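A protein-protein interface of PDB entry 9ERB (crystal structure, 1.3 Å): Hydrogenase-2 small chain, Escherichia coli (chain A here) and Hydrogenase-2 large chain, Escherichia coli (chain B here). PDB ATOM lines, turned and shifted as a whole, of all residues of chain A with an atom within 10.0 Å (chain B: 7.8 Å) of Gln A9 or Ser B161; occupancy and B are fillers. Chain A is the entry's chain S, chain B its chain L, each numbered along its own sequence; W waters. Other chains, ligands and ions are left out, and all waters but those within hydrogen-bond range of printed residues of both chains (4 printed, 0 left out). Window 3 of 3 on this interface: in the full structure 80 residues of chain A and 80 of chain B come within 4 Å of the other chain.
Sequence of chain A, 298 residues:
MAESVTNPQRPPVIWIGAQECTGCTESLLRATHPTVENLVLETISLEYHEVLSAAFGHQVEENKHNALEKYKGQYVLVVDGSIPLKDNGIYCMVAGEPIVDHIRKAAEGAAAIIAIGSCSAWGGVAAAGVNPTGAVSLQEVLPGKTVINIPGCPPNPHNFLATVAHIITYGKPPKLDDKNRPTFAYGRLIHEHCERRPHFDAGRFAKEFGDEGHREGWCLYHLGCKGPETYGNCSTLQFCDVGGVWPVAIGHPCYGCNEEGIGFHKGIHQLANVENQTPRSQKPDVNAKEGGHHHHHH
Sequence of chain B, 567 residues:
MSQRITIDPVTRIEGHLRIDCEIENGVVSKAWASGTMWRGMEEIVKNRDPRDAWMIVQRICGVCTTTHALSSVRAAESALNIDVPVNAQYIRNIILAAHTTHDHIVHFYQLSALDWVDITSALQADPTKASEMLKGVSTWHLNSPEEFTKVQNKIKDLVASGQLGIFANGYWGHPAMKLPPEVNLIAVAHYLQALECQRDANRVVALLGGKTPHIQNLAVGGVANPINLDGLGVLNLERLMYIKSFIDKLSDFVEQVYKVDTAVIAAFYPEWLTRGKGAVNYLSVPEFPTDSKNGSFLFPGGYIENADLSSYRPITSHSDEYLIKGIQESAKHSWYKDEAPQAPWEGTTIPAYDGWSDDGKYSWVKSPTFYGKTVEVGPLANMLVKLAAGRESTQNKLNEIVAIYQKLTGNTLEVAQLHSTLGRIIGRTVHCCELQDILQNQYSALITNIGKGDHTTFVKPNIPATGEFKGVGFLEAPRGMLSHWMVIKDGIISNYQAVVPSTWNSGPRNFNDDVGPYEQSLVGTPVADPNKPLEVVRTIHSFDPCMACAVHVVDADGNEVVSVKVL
The side-chain amide nitrogen of Gln A9 is in hydrogen-bond range of the backbone carbonyl oxygen of Ser B161 (2.9 Å). The side-chain amide oxygen (OE1) of Gln A9 sits close to the side-chain amide oxygen (OE1) of Gln B163. The guanidinium group (NH2) of Arg A10 sits at hydrogen-bond distance from the side-chain hydroxyl (OG) of Ser B161 (3.2 Å). N of Arg A10 is in hydrogen-bond range of OE1 of Gln B163. The side-chain amide nitrogen of Gln B163 lies within hydrogen-bond range of the side-chain hydroxyl of Tyr A71 (3.1 Å).
The backbone carbonyl oxygen of Val A40 lies within hydrogen-bond range of the guanidinium group of Arg A10 (3.2 Å). NH1 of Arg A10 sits at hydrogen-bond distance from O of Ile A44 (2.9 Å). OH of Tyr A71 is in hydrogen-bond range of OE2 of Glu A47. The side-chain hydroxyl of Tyr A71 is in hydrogen-bond range of the side-chain amino group of Lys A70. OG of Ser B161 is in hydrogen-bond range of O of Leu B158. The side-chain hydroxyl (OG) of Ser B161 sits at hydrogen-bond distance from the backbone NH (N) of Gln B163 (3.0 Å).
Among the printed residues, merely in contact across the chains: Leu A41 with Leu B158 (3.7 Å), Ser A45 with Gln B163 (3.5 Å), Leu A46 with Gly B165 (3.2 Å) and Lys A70 with Gly B162 (3.6 Å).
Gln A9 touches just these residues of chain B: Ser B161 (2.9 Å) and Gln B163 (3.2 Å). Ser B161 touches just these residues of chain A: Gln A9 (2.9 Å) and Arg A10 (3.2 Å). Of chain A, only Leu A41 comes within 4 Å of Leu B158. Gly B162 touches just one residue of chain A: Lys A70. Gln B163 touches just these residues of chain A: Gln A9, Arg A10, Ser A45 and Tyr A71. Of the printed residues of chain B, Arg A10 touches Ser B161 (3.2 Å) and Gln B163 (2.8 Å). Of the printed residues of chain B, Leu A46 touches Gly B165 (3.2 Å). Printed residues of chain B within 4 Å of Lys A70: Gly B162. Of the printed residues of chain B, Tyr A71 touches Gln B163. Of the printed residues of chain B, Ser A45 touches Gln B163 (3.5 Å). Glu A47 touches none of the printed residues of chain B. Ile A168 touches none of the printed residues of chain B.
Printed residues of chain B that touch a printed residue of chain A: Leu B158, Ser B161, Gly B162, Gln B163 and Gly B165. Printed residues of chain A that touch a printed residue of chain B: Gln A9, Arg A10, Leu A41, Ser A45, Leu A46, Lys A70 and Tyr A71. Among the printed residues, no Asp or Glu carboxylate lies within 4 Å of a Lys or Arg side-chain nitrogen of the other chain.
Water W3 lies within hydrogen-bond range of OG of Ser A45 (2.7 Å), O of Gln B163 (2.7 Å), NH1 of Arg A10 (3.0 Å) and N of Gly B165 (3.2 Å). Water W4 lies within hydrogen-bond range of O of Pro A8 (2.7 Å), OE1 of Gln B163 (2.8 Å), NE of Arg A10 (2.9 Å) and OG of Ser B161 (3.4 Å). Water W1 lies within hydrogen-bond range of OE1 of Gln A9 (2.7 Å), NZ of Lys A70 (2.8 Å) and O of Ser B161 (3.4 Å). Water W2 bridges the guanidinium group (NH2) of Arg A10 and the backbone carbonyl oxygen (O) of Asp B157.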
ATOM      1  N   PRO A   8       9.710  -0.153 -26.146  1.00  0.00           N
ATOM      2  CA  PRO A   8      11.138  -0.175 -26.485  1.00  0.00           C
ATOM      3  C   PRO A   8      11.796  -1.474 -26.042  1.00  0.00           C
ATOM      4  O   PRO A   8      11.297  -2.130 -25.110  1.00  0.00           O
ATOM      5  CB  PRO A   8      11.700   1.005 -25.689  1.00  0.00           C
ATOM      6  CG  PRO A   8      10.824   1.079 -24.488  1.00  0.00           C
ATOM      7  CD  PRO A   8       9.442   0.685 -24.964  1.00  0.00           C
ATOM      8  N   GLN A   9      12.890  -1.843 -26.698  1.00  0.00           N
ATOM      9  CA  GLN A   9      13.663  -2.995 -26.250  1.00  0.00           C
ATOM     10  C   GLN A   9      14.348  -2.664 -24.927  1.00  0.00           C
ATOM     11  O   GLN A   9      14.654  -1.501 -24.635  1.00  0.00           O
ATOM     12  CB  GLN A   9      14.708  -3.373 -27.289  1.00  0.00           C
ATOM     13  CG  GLN A   9      14.088  -3.801 -28.616  1.00  0.00           C
ATOM     14  CD  GLN A   9      13.344  -5.111 -28.509  1.00  0.00           C
ATOM     15  OE1 GLN A   9      13.951  -6.157 -28.352  1.00  0.00           O
ATOM     16  NE2 GLN A   9      12.019  -5.055 -28.581  1.00  0.00           N
ATOM     17  N   ARG A  10      14.566  -3.713 -24.102  1.00  0.00           N
ATOM     18  CA  ARG A  10      15.192  -3.597 -22.793  1.00  0.00           C
ATOM     19  C   ARG A  10      16.536  -4.298 -22.782  1.00  0.00           C
ATOM     20  O   ARG A  10      16.743  -5.287 -23.497  1.00  0.00           O
ATOM     21  CB  ARG A  10      14.280  -4.181 -21.704  1.00  0.00           C
ATOM     22  CG  ARG A  10      13.005  -3.390 -21.462  1.00  0.00           C
ATOM     23  CD  ARG A  10      11.934  -4.184 -20.704  1.00  0.00           C
ATOM     24  NE  ARG A  10      11.206  -5.079 -21.600  1.00  0.00           N
ATOM     25  CZ  ARG A  10      11.090  -6.388 -21.473  1.00  0.00           C
ATOM     26  NH1 ARG A  10      11.544  -7.030 -20.396  1.00  0.00           N
ATOM     27  NH2 ARG A  10      10.476  -7.075 -22.431  1.00  0.00           N
ATOM     28  N   PRO A  11      17.477  -3.814 -21.985  1.00  0.00           N
ATOM     29  CA  PRO A  11      18.813  -4.401 -21.978  1.00  0.00           C
ATOM     30  C   PRO A  11      18.797  -5.796 -21.383  1.00  0.00           C
ATOM     31  O   PRO A  11      18.140  -6.034 -20.357  1.00  0.00           O
ATOM     32  CB  PRO A  11      19.634  -3.436 -21.112  1.00  0.00           C
ATOM     33  CG  PRO A  11      18.659  -2.558 -20.429  1.00  0.00           C
ATOM     34  CD  PRO A  11      17.400  -2.553 -21.231  1.00  0.00           C
ATOM     35  N   PRO A  12      19.492  -6.740 -22.009  1.00  0.00           N
ATOM     36  CA  PRO A  12      19.428  -8.137 -21.589  1.00  0.00           C
ATOM     37  C   PRO A  12      20.394  -8.471 -20.463  1.00  0.00           C
ATOM     38  O   PRO A  12      21.509  -7.948 -20.371  1.00  0.00           O
ATOM     39  CB  PRO A  12      19.863  -8.897 -22.858  1.00  0.00           C
ATOM     40  CG  PRO A  12      20.778  -7.961 -23.550  1.00  0.00           C
ATOM     41  CD  PRO A  12      20.209  -6.582 -23.294  1.00  0.00           C
ATOM     42  N   VAL A  40      11.982  -6.790 -14.065  1.00  0.00           N
ATOM     43  CA  VAL A  40      11.892  -7.767 -15.132  1.00  0.00           C
ATOM     44  C   VAL A  40      10.914  -7.344 -16.226  1.00  0.00           C
ATOM     45  O   VAL A  40      11.041  -7.857 -17.356  1.00  0.00           O
ATOM     46  CB  VAL A  40      11.577  -9.185 -14.624  1.00  0.00           C
ATOM     47  CG1 VAL A  40      12.609  -9.655 -13.634  1.00  0.00           C
ATOM     48  CG2 VAL A  40      10.193  -9.297 -14.060  1.00  0.00           C
ATOM     49  N   LEU A  41       9.971  -6.447 -15.960  1.00  0.00           N
ATOM     50  CA  LEU A  41       9.032  -6.025 -17.002  1.00  0.00           C
ATOM     51  C   LEU A  41       9.434  -4.716 -17.656  1.00  0.00           C
ATOM     52  O   LEU A  41       9.076  -4.493 -18.824  1.00  0.00           O
ATOM     53  CB  LEU A  41       7.614  -5.888 -16.429  1.00  0.00           C
ATOM     54  CG  LEU A  41       6.972  -7.188 -15.933  1.00  0.00           C
ATOM     55  CD1 LEU A  41       5.579  -6.883 -15.410  1.00  0.00           C
ATOM     56  CD2 LEU A  41       6.926  -8.273 -16.982  1.00  0.00           C
ATOM     57  N   GLU A  42      10.191  -3.857 -16.970  1.00  0.00           N
ATOM     58  CA  GLU A  42      10.470  -2.514 -17.470  1.00  0.00           C
ATOM     59  C   GLU A  42      11.954  -2.215 -17.605  1.00  0.00           C
ATOM     60  O   GLU A  42      12.388  -1.668 -18.626  1.00  0.00           O
ATOM     61  CB  GLU A  42       9.839  -1.463 -16.535  1.00  0.00           C
ATOM     62  CG  GLU A  42       8.425  -1.786 -16.059  1.00  0.00           C
ATOM     63  CD  GLU A  42       7.348  -1.491 -17.088  1.00  0.00           C
ATOM     64  OE1 GLU A  42       7.670  -0.967 -18.175  1.00  0.00           O
ATOM     65  OE2 GLU A  42       6.173  -1.801 -16.796  1.00  0.00           O
ATOM     66  N   THR A  43      12.756  -2.542 -16.599  1.00  0.00           N
ATOM     67  CA  THR A  43      14.146  -2.106 -16.609  1.00  0.00           C
ATOM     68  C   THR A  43      15.041  -2.959 -17.506  1.00  0.00           C
ATOM     69  O   THR A  43      15.869  -2.432 -18.267  1.00  0.00           O
ATOM     70  CB  THR A  43      14.703  -2.129 -15.188  1.00  0.00           C
ATOM     71  OG1 THR A  43      13.771  -1.466 -14.329  1.00  0.00           O
ATOM     72  CG2 THR A  43      16.087  -1.428 -15.142  1.00  0.00           C
ATOM     73  N   ILE A  44      14.948  -4.280 -17.389  1.00  0.00           N
ATOM     74  CA  ILE A  44      15.791  -5.217 -18.128  1.00  0.00           C
ATOM     75  C   ILE A  44      14.913  -6.255 -18.807  1.00  0.00           C
ATOM     76  O   ILE A  44      13.708  -6.348 -18.566  1.00  0.00           O
ATOM     77  CB  ILE A  44      16.836  -5.922 -17.226  1.00  0.00           C
ATOM     78  CG1 ILE A  44      16.128  -6.786 -16.161  1.00  0.00           C
ATOM     79  CG2 ILE A  44      17.794  -4.894 -16.579  1.00  0.00           C
ATOM     80  CD1 ILE A  44      17.019  -7.746 -15.426  1.00  0.00           C
ATOM     81  N   SER A  45      15.544  -7.041 -19.668  1.00  0.00           N
ATOM     82  CA  SER A  45      15.007  -8.327 -20.072  1.00  0.00           C
ATOM     83  C   SER A  45      15.875  -9.398 -19.420  1.00  0.00           C
ATOM     84  O   SER A  45      17.036  -9.572 -19.783  1.00  0.00           O
ATOM     85  CB  SER A  45      14.985  -8.504 -21.581  1.00  0.00           C
ATOM     86  OG  SER A  45      14.245  -9.679 -21.860  1.00  0.00           O
ATOM     87  N   LEU A  46      15.287 -10.136 -18.478  1.00  0.00           N
ATOM     88  CA  LEU A  46      15.987 -11.201 -17.766  1.00  0.00           C
ATOM     89  C   LEU A  46      15.861 -12.441 -18.635  1.00  0.00           C
ATOM     90  O   LEU A  46      14.880 -13.197 -18.568  1.00  0.00           O
ATOM     91  CB  LEU A  46      15.375 -11.407 -16.391  1.00  0.00           C
ATOM     92  CG  LEU A  46      16.085 -12.361 -15.426  1.00  0.00           C
ATOM     93  CD1 LEU A  46      17.552 -12.018 -15.272  1.00  0.00           C
ATOM     94  CD2 LEU A  46      15.368 -12.361 -14.085  1.00  0.00           C
ATOM     95  N   GLU A  47      16.885 -12.655 -19.463  1.00  0.00           N
ATOM     96  CA  GLU A  47      16.854 -13.699 -20.485  1.00  0.00           C
ATOM     97  C   GLU A  47      17.221 -15.066 -19.965  1.00  0.00           C
ATOM     98  O   GLU A  47      16.931 -16.066 -20.635  1.00  0.00           O
ATOM     99  CB  GLU A  47      17.807 -13.334 -21.628  1.00  0.00           C
ATOM    100  CG  GLU A  47      17.475 -12.060 -22.280  1.00  0.00           C
ATOM    101  CD  GLU A  47      16.406 -12.211 -23.292  1.00  0.00           C
ATOM    102  OE1 GLU A  47      16.216 -13.353 -23.782  1.00  0.00           O
ATOM    103  OE2 GLU A  47      15.787 -11.204 -23.634  1.00  0.00           O
ATOM    104  N   LYS A  70      21.741 -14.013 -29.735  1.00  0.00           N
ATOM    105  CA  LYS A  70      20.991 -12.811 -30.099  1.00  0.00           C
ATOM    106  C   LYS A  70      21.620 -11.563 -29.499  1.00  0.00           C
ATOM    107  O   LYS A  70      21.650 -10.505 -30.139  1.00  0.00           O
ATOM    108  CB  LYS A  70      19.538 -12.943 -29.644  1.00  0.00           C
ATOM    109  CG  LYS A  70      18.654 -11.700 -29.874  1.00  0.00           C
ATOM    110  CD  LYS A  70      17.184 -11.989 -29.517  1.00  0.00           C
ATOM    111  CE  LYS A  70      16.263 -10.804 -29.717  1.00  0.00           C
ATOM    112  NZ  LYS A  70      14.867 -11.074 -29.225  1.00  0.00           N
ATOM    113  N   TYR A  71      22.150 -11.669 -28.277  1.00  0.00           N
ATOM    114  CA  TYR A  71      22.619 -10.522 -27.513  1.00  0.00           C
ATOM    115  C   TYR A  71      24.129 -10.524 -27.313  1.00  0.00           C
ATOM    116  O   TYR A  71      24.628  -9.860 -26.403  1.00  0.00           O
ATOM    117  CB  TYR A  71      21.894 -10.491 -26.171  1.00  0.00           C
ATOM    118  CG  TYR A  71      20.393 -10.318 -26.249  1.00  0.00           C
ATOM    119  CD1 TYR A  71      19.821  -9.164 -26.766  1.00  0.00           C
ATOM    120  CD2 TYR A  71      19.548 -11.339 -25.855  1.00  0.00           C
ATOM    121  CE1 TYR A  71      18.453  -9.018 -26.813  1.00  0.00           C
ATOM    122  CE2 TYR A  71      18.188 -11.211 -25.895  1.00  0.00           C
ATOM    123  CZ  TYR A  71      17.640 -10.050 -26.388  1.00  0.00           C
ATOM    124  OH  TYR A  71      16.263  -9.914 -26.442  1.00  0.00           O
ATOM    125  N   GLN A  74      26.273  -7.645 -25.707  1.00  0.00           N
ATOM    126  CA  GLN A  74      25.316  -6.694 -25.179  1.00  0.00           C
ATOM    127  C   GLN A  74      24.794  -7.008 -23.781  1.00  0.00           C
ATOM    128  O   GLN A  74      24.296  -6.089 -23.123  1.00  0.00           O
ATOM    129  CB  GLN A  74      24.093  -6.600 -26.104  1.00  0.00           C
ATOM    130  CG  GLN A  74      24.438  -6.187 -27.522  1.00  0.00           C
ATOM    131  CD  GLN A  74      23.209  -6.017 -28.396  1.00  0.00           C
ATOM    132  OE1 GLN A  74      22.232  -6.754 -28.268  1.00  0.00           O
ATOM    133  NE2 GLN A  74      23.272  -5.065 -29.326  1.00  0.00           N
ATOM    134  N   ILE A 168      23.195   1.063 -17.730  1.00  0.00           N
ATOM    135  CA  ILE A 168      22.133   1.318 -18.699  1.00  0.00           C
ATOM    136  C   ILE A 168      22.015   2.810 -19.008  1.00  0.00           C
ATOM    137  O   ILE A 168      21.891   3.220 -20.177  1.00  0.00           O
ATOM    138  CB  ILE A 168      20.791   0.773 -18.172  1.00  0.00           C
ATOM    139  CG1 ILE A 168      20.816  -0.742 -18.062  1.00  0.00           C
ATOM    140  CG2 ILE A 168      19.634   1.275 -19.055  1.00  0.00           C
ATOM    141  CD1 ILE A 168      19.646  -1.279 -17.205  1.00  0.00           C
ATOM    142  N   ILE B 155       1.143  -8.010 -19.996  1.00  0.00           N
ATOM    143  CA  ILE B 155       1.575  -9.227 -20.679  1.00  0.00           C
ATOM    144  C   ILE B 155       1.634  -8.995 -22.181  1.00  0.00           C
ATOM    145  O   ILE B 155       2.553  -9.452 -22.865  1.00  0.00           O
ATOM    146  CB  ILE B 155       0.626 -10.398 -20.409  1.00  0.00           C
ATOM    147  CG1 ILE B 155       0.403 -10.698 -18.943  1.00  0.00           C
ATOM    148  CG2 ILE B 155       1.178 -11.643 -21.113  1.00  0.00           C
ATOM    149  CD1 ILE B 155      -0.846 -11.591 -18.779  1.00  0.00           C
ATOM    150  N   LYS B 156       0.611  -8.348 -22.722  1.00  0.00           N
ATOM    151  CA  LYS B 156       0.560  -8.106 -24.155  1.00  0.00           C
ATOM    152  C   LYS B 156       1.799  -7.353 -24.611  1.00  0.00           C
ATOM    153  O   LYS B 156       2.423  -7.715 -25.611  1.00  0.00           O
ATOM    154  CB  LYS B 156      -0.680  -7.275 -24.454  1.00  0.00           C
ATOM    155  CG  LYS B 156      -1.039  -7.117 -25.932  1.00  0.00           C
ATOM    156  CD  LYS B 156      -2.472  -6.554 -26.126  1.00  0.00           C
ATOM    157  CE  LYS B 156      -3.445  -7.050 -25.060  1.00  0.00           C
ATOM    158  NZ  LYS B 156      -4.767  -7.445 -25.616  1.00  0.00           N
ATOM    159  N   ASP B 157       2.161  -6.306 -23.889  1.00  0.00           N
ATOM    160  CA  ASP B 157       3.322  -5.507 -24.259  1.00  0.00           C
ATOM    161  C   ASP B 157       4.593  -6.332 -24.196  1.00  0.00           C
ATOM    162  O   ASP B 157       5.420  -6.278 -25.110  1.00  0.00           O
ATOM    163  CB  ASP B 157       3.426  -4.293 -23.341  1.00  0.00           C
ATOM    164  CG  ASP B 157       2.357  -3.241 -23.611  1.00  0.00           C
ATOM    165  OD1 ASP B 157       1.637  -3.333 -24.623  1.00  0.00           O
ATOM    166  OD2 ASP B 157       2.263  -2.324 -22.786  1.00  0.00           O
ATOM    167  N   LEU B 158       4.749  -7.147 -23.149  1.00  0.00           N
ATOM    168  CA  LEU B 158       5.943  -7.982 -23.054  1.00  0.00           C
ATOM    169  C   LEU B 158       6.030  -8.934 -24.244  1.00  0.00           C
ATOM    170  O   LEU B 158       7.082  -9.063 -24.878  1.00  0.00           O
ATOM    171  CB  LEU B 158       5.949  -8.723 -21.712  1.00  0.00           C
ATOM    172  CG  LEU B 158       7.110  -9.708 -21.549  1.00  0.00           C
ATOM    173  CD1 LEU B 158       7.901  -9.477 -20.294  1.00  0.00           C
ATOM    174  CD2 LEU B 158       6.550 -11.109 -21.601  1.00  0.00           C
ATOM    175  N   VAL B 159       4.922  -9.599 -24.582  1.00  0.00           N
ATOM    176  CA  VAL B 159       4.952 -10.552 -25.697  1.00  0.00           C
ATOM    177  C   VAL B 159       5.250  -9.813 -26.996  1.00  0.00           C
ATOM    178  O   VAL B 159       6.059 -10.268 -27.825  1.00  0.00           O
ATOM    179  CB  VAL B 159       3.621 -11.327 -25.770  1.00  0.00           C
ATOM    180  CG1 VAL B 159       3.495 -12.111 -27.106  1.00  0.00           C
ATOM    181  CG2 VAL B 159       3.464 -12.264 -24.580  1.00  0.00           C
ATOM    182  N   ALA B 160       4.654  -8.636 -27.157  1.00  0.00           N
ATOM    183  CA  ALA B 160       4.840  -7.858 -28.380  1.00  0.00           C
ATOM    184  C   ALA B 160       6.285  -7.426 -28.554  1.00  0.00           C
ATOM    185  O   ALA B 160       6.765  -7.328 -29.684  1.00  0.00           O
ATOM    186  CB  ALA B 160       3.936  -6.629 -28.367  1.00  0.00           C
ATOM    187  N   SER B 161       6.994  -7.180 -27.451  1.00  0.00           N
ATOM    188  CA  SER B 161       8.393  -6.765 -27.528  1.00  0.00           C
ATOM    189  C   SER B 161       9.293  -7.831 -28.114  1.00  0.00           C
ATOM    190  O   SER B 161      10.423  -7.527 -28.540  1.00  0.00           O
ATOM    191  CB  SER B 161       8.893  -6.394 -26.133  1.00  0.00           C
ATOM    192  OG  SER B 161       9.263  -7.541 -25.361  1.00  0.00           O
ATOM    193  N   GLY B 162       8.849  -9.077 -28.133  1.00  0.00           N
ATOM    194  CA  GLY B 162       9.718 -10.155 -28.530  1.00  0.00           C
ATOM    195  C   GLY B 162      10.771 -10.531 -27.512  1.00  0.00           C
ATOM    196  O   GLY B 162      11.616 -11.378 -27.811  1.00  0.00           O
ATOM    197  N   GLN B 163      10.763  -9.905 -26.336  1.00  0.00           N
ATOM    198  CA  GLN B 163      11.699 -10.171 -25.244  1.00  0.00           C
ATOM    199  C   GLN B 163      10.863 -10.752 -24.108  1.00  0.00           C
ATOM    200  O   GLN B 163      10.410 -10.050 -23.210  1.00  0.00           O
ATOM    201  CB  GLN B 163      12.436  -8.960 -24.784  1.00  0.00           C
ATOM    202  CG  GLN B 163      13.241  -8.288 -25.849  1.00  0.00           C
ATOM    203  CD  GLN B 163      13.997  -7.102 -25.285  1.00  0.00           C
ATOM    204  OE1 GLN B 163      13.382  -6.096 -24.925  1.00  0.00           O
ATOM    205  NE2 GLN B 163      15.307  -7.253 -25.106  1.00  0.00           N
ATOM    206  N   LEU B 164      10.624 -12.063 -24.179  1.00  0.00           N
ATOM    207  CA  LEU B 164       9.741 -12.703 -23.219  1.00  0.00           C
ATOM    208  C   LEU B 164      10.437 -13.005 -21.898  1.00  0.00           C
ATOM    209  O   LEU B 164       9.744 -13.222 -20.904  1.00  0.00           O
ATOM    210  CB  LEU B 164       9.133 -13.994 -23.783  1.00  0.00           C
ATOM    211  CG  LEU B 164       7.800 -13.768 -24.522  1.00  0.00           C
ATOM    212  CD1 LEU B 164       8.046 -13.025 -25.825  1.00  0.00           C
ATOM    213  CD2 LEU B 164       7.115 -15.096 -24.808  1.00  0.00           C
ATOM    214  N   GLY B 165      11.759 -12.992 -21.861  1.00  0.00           N
ATOM    215  CA  GLY B 165      12.448 -13.092 -20.575  1.00  0.00           C
ATOM    216  C   GLY B 165      12.077 -14.362 -19.832  1.00  0.00           C
ATOM    217  O   GLY B 165      12.150 -15.465 -20.384  1.00  0.00           O
HETATM  218  O   HOH W   1      13.460  -8.617 -29.457  1.00  0.00           O
HETATM  219  O   HOH W   2       7.994  -4.990 -23.199  1.00  0.00           O
HETATM  220  O   HOH W   3      11.785  -9.934 -20.856  1.00  0.00           O
HETATM  221  O   HOH W   4      11.025  -4.742 -24.454  1.00  0.00           O
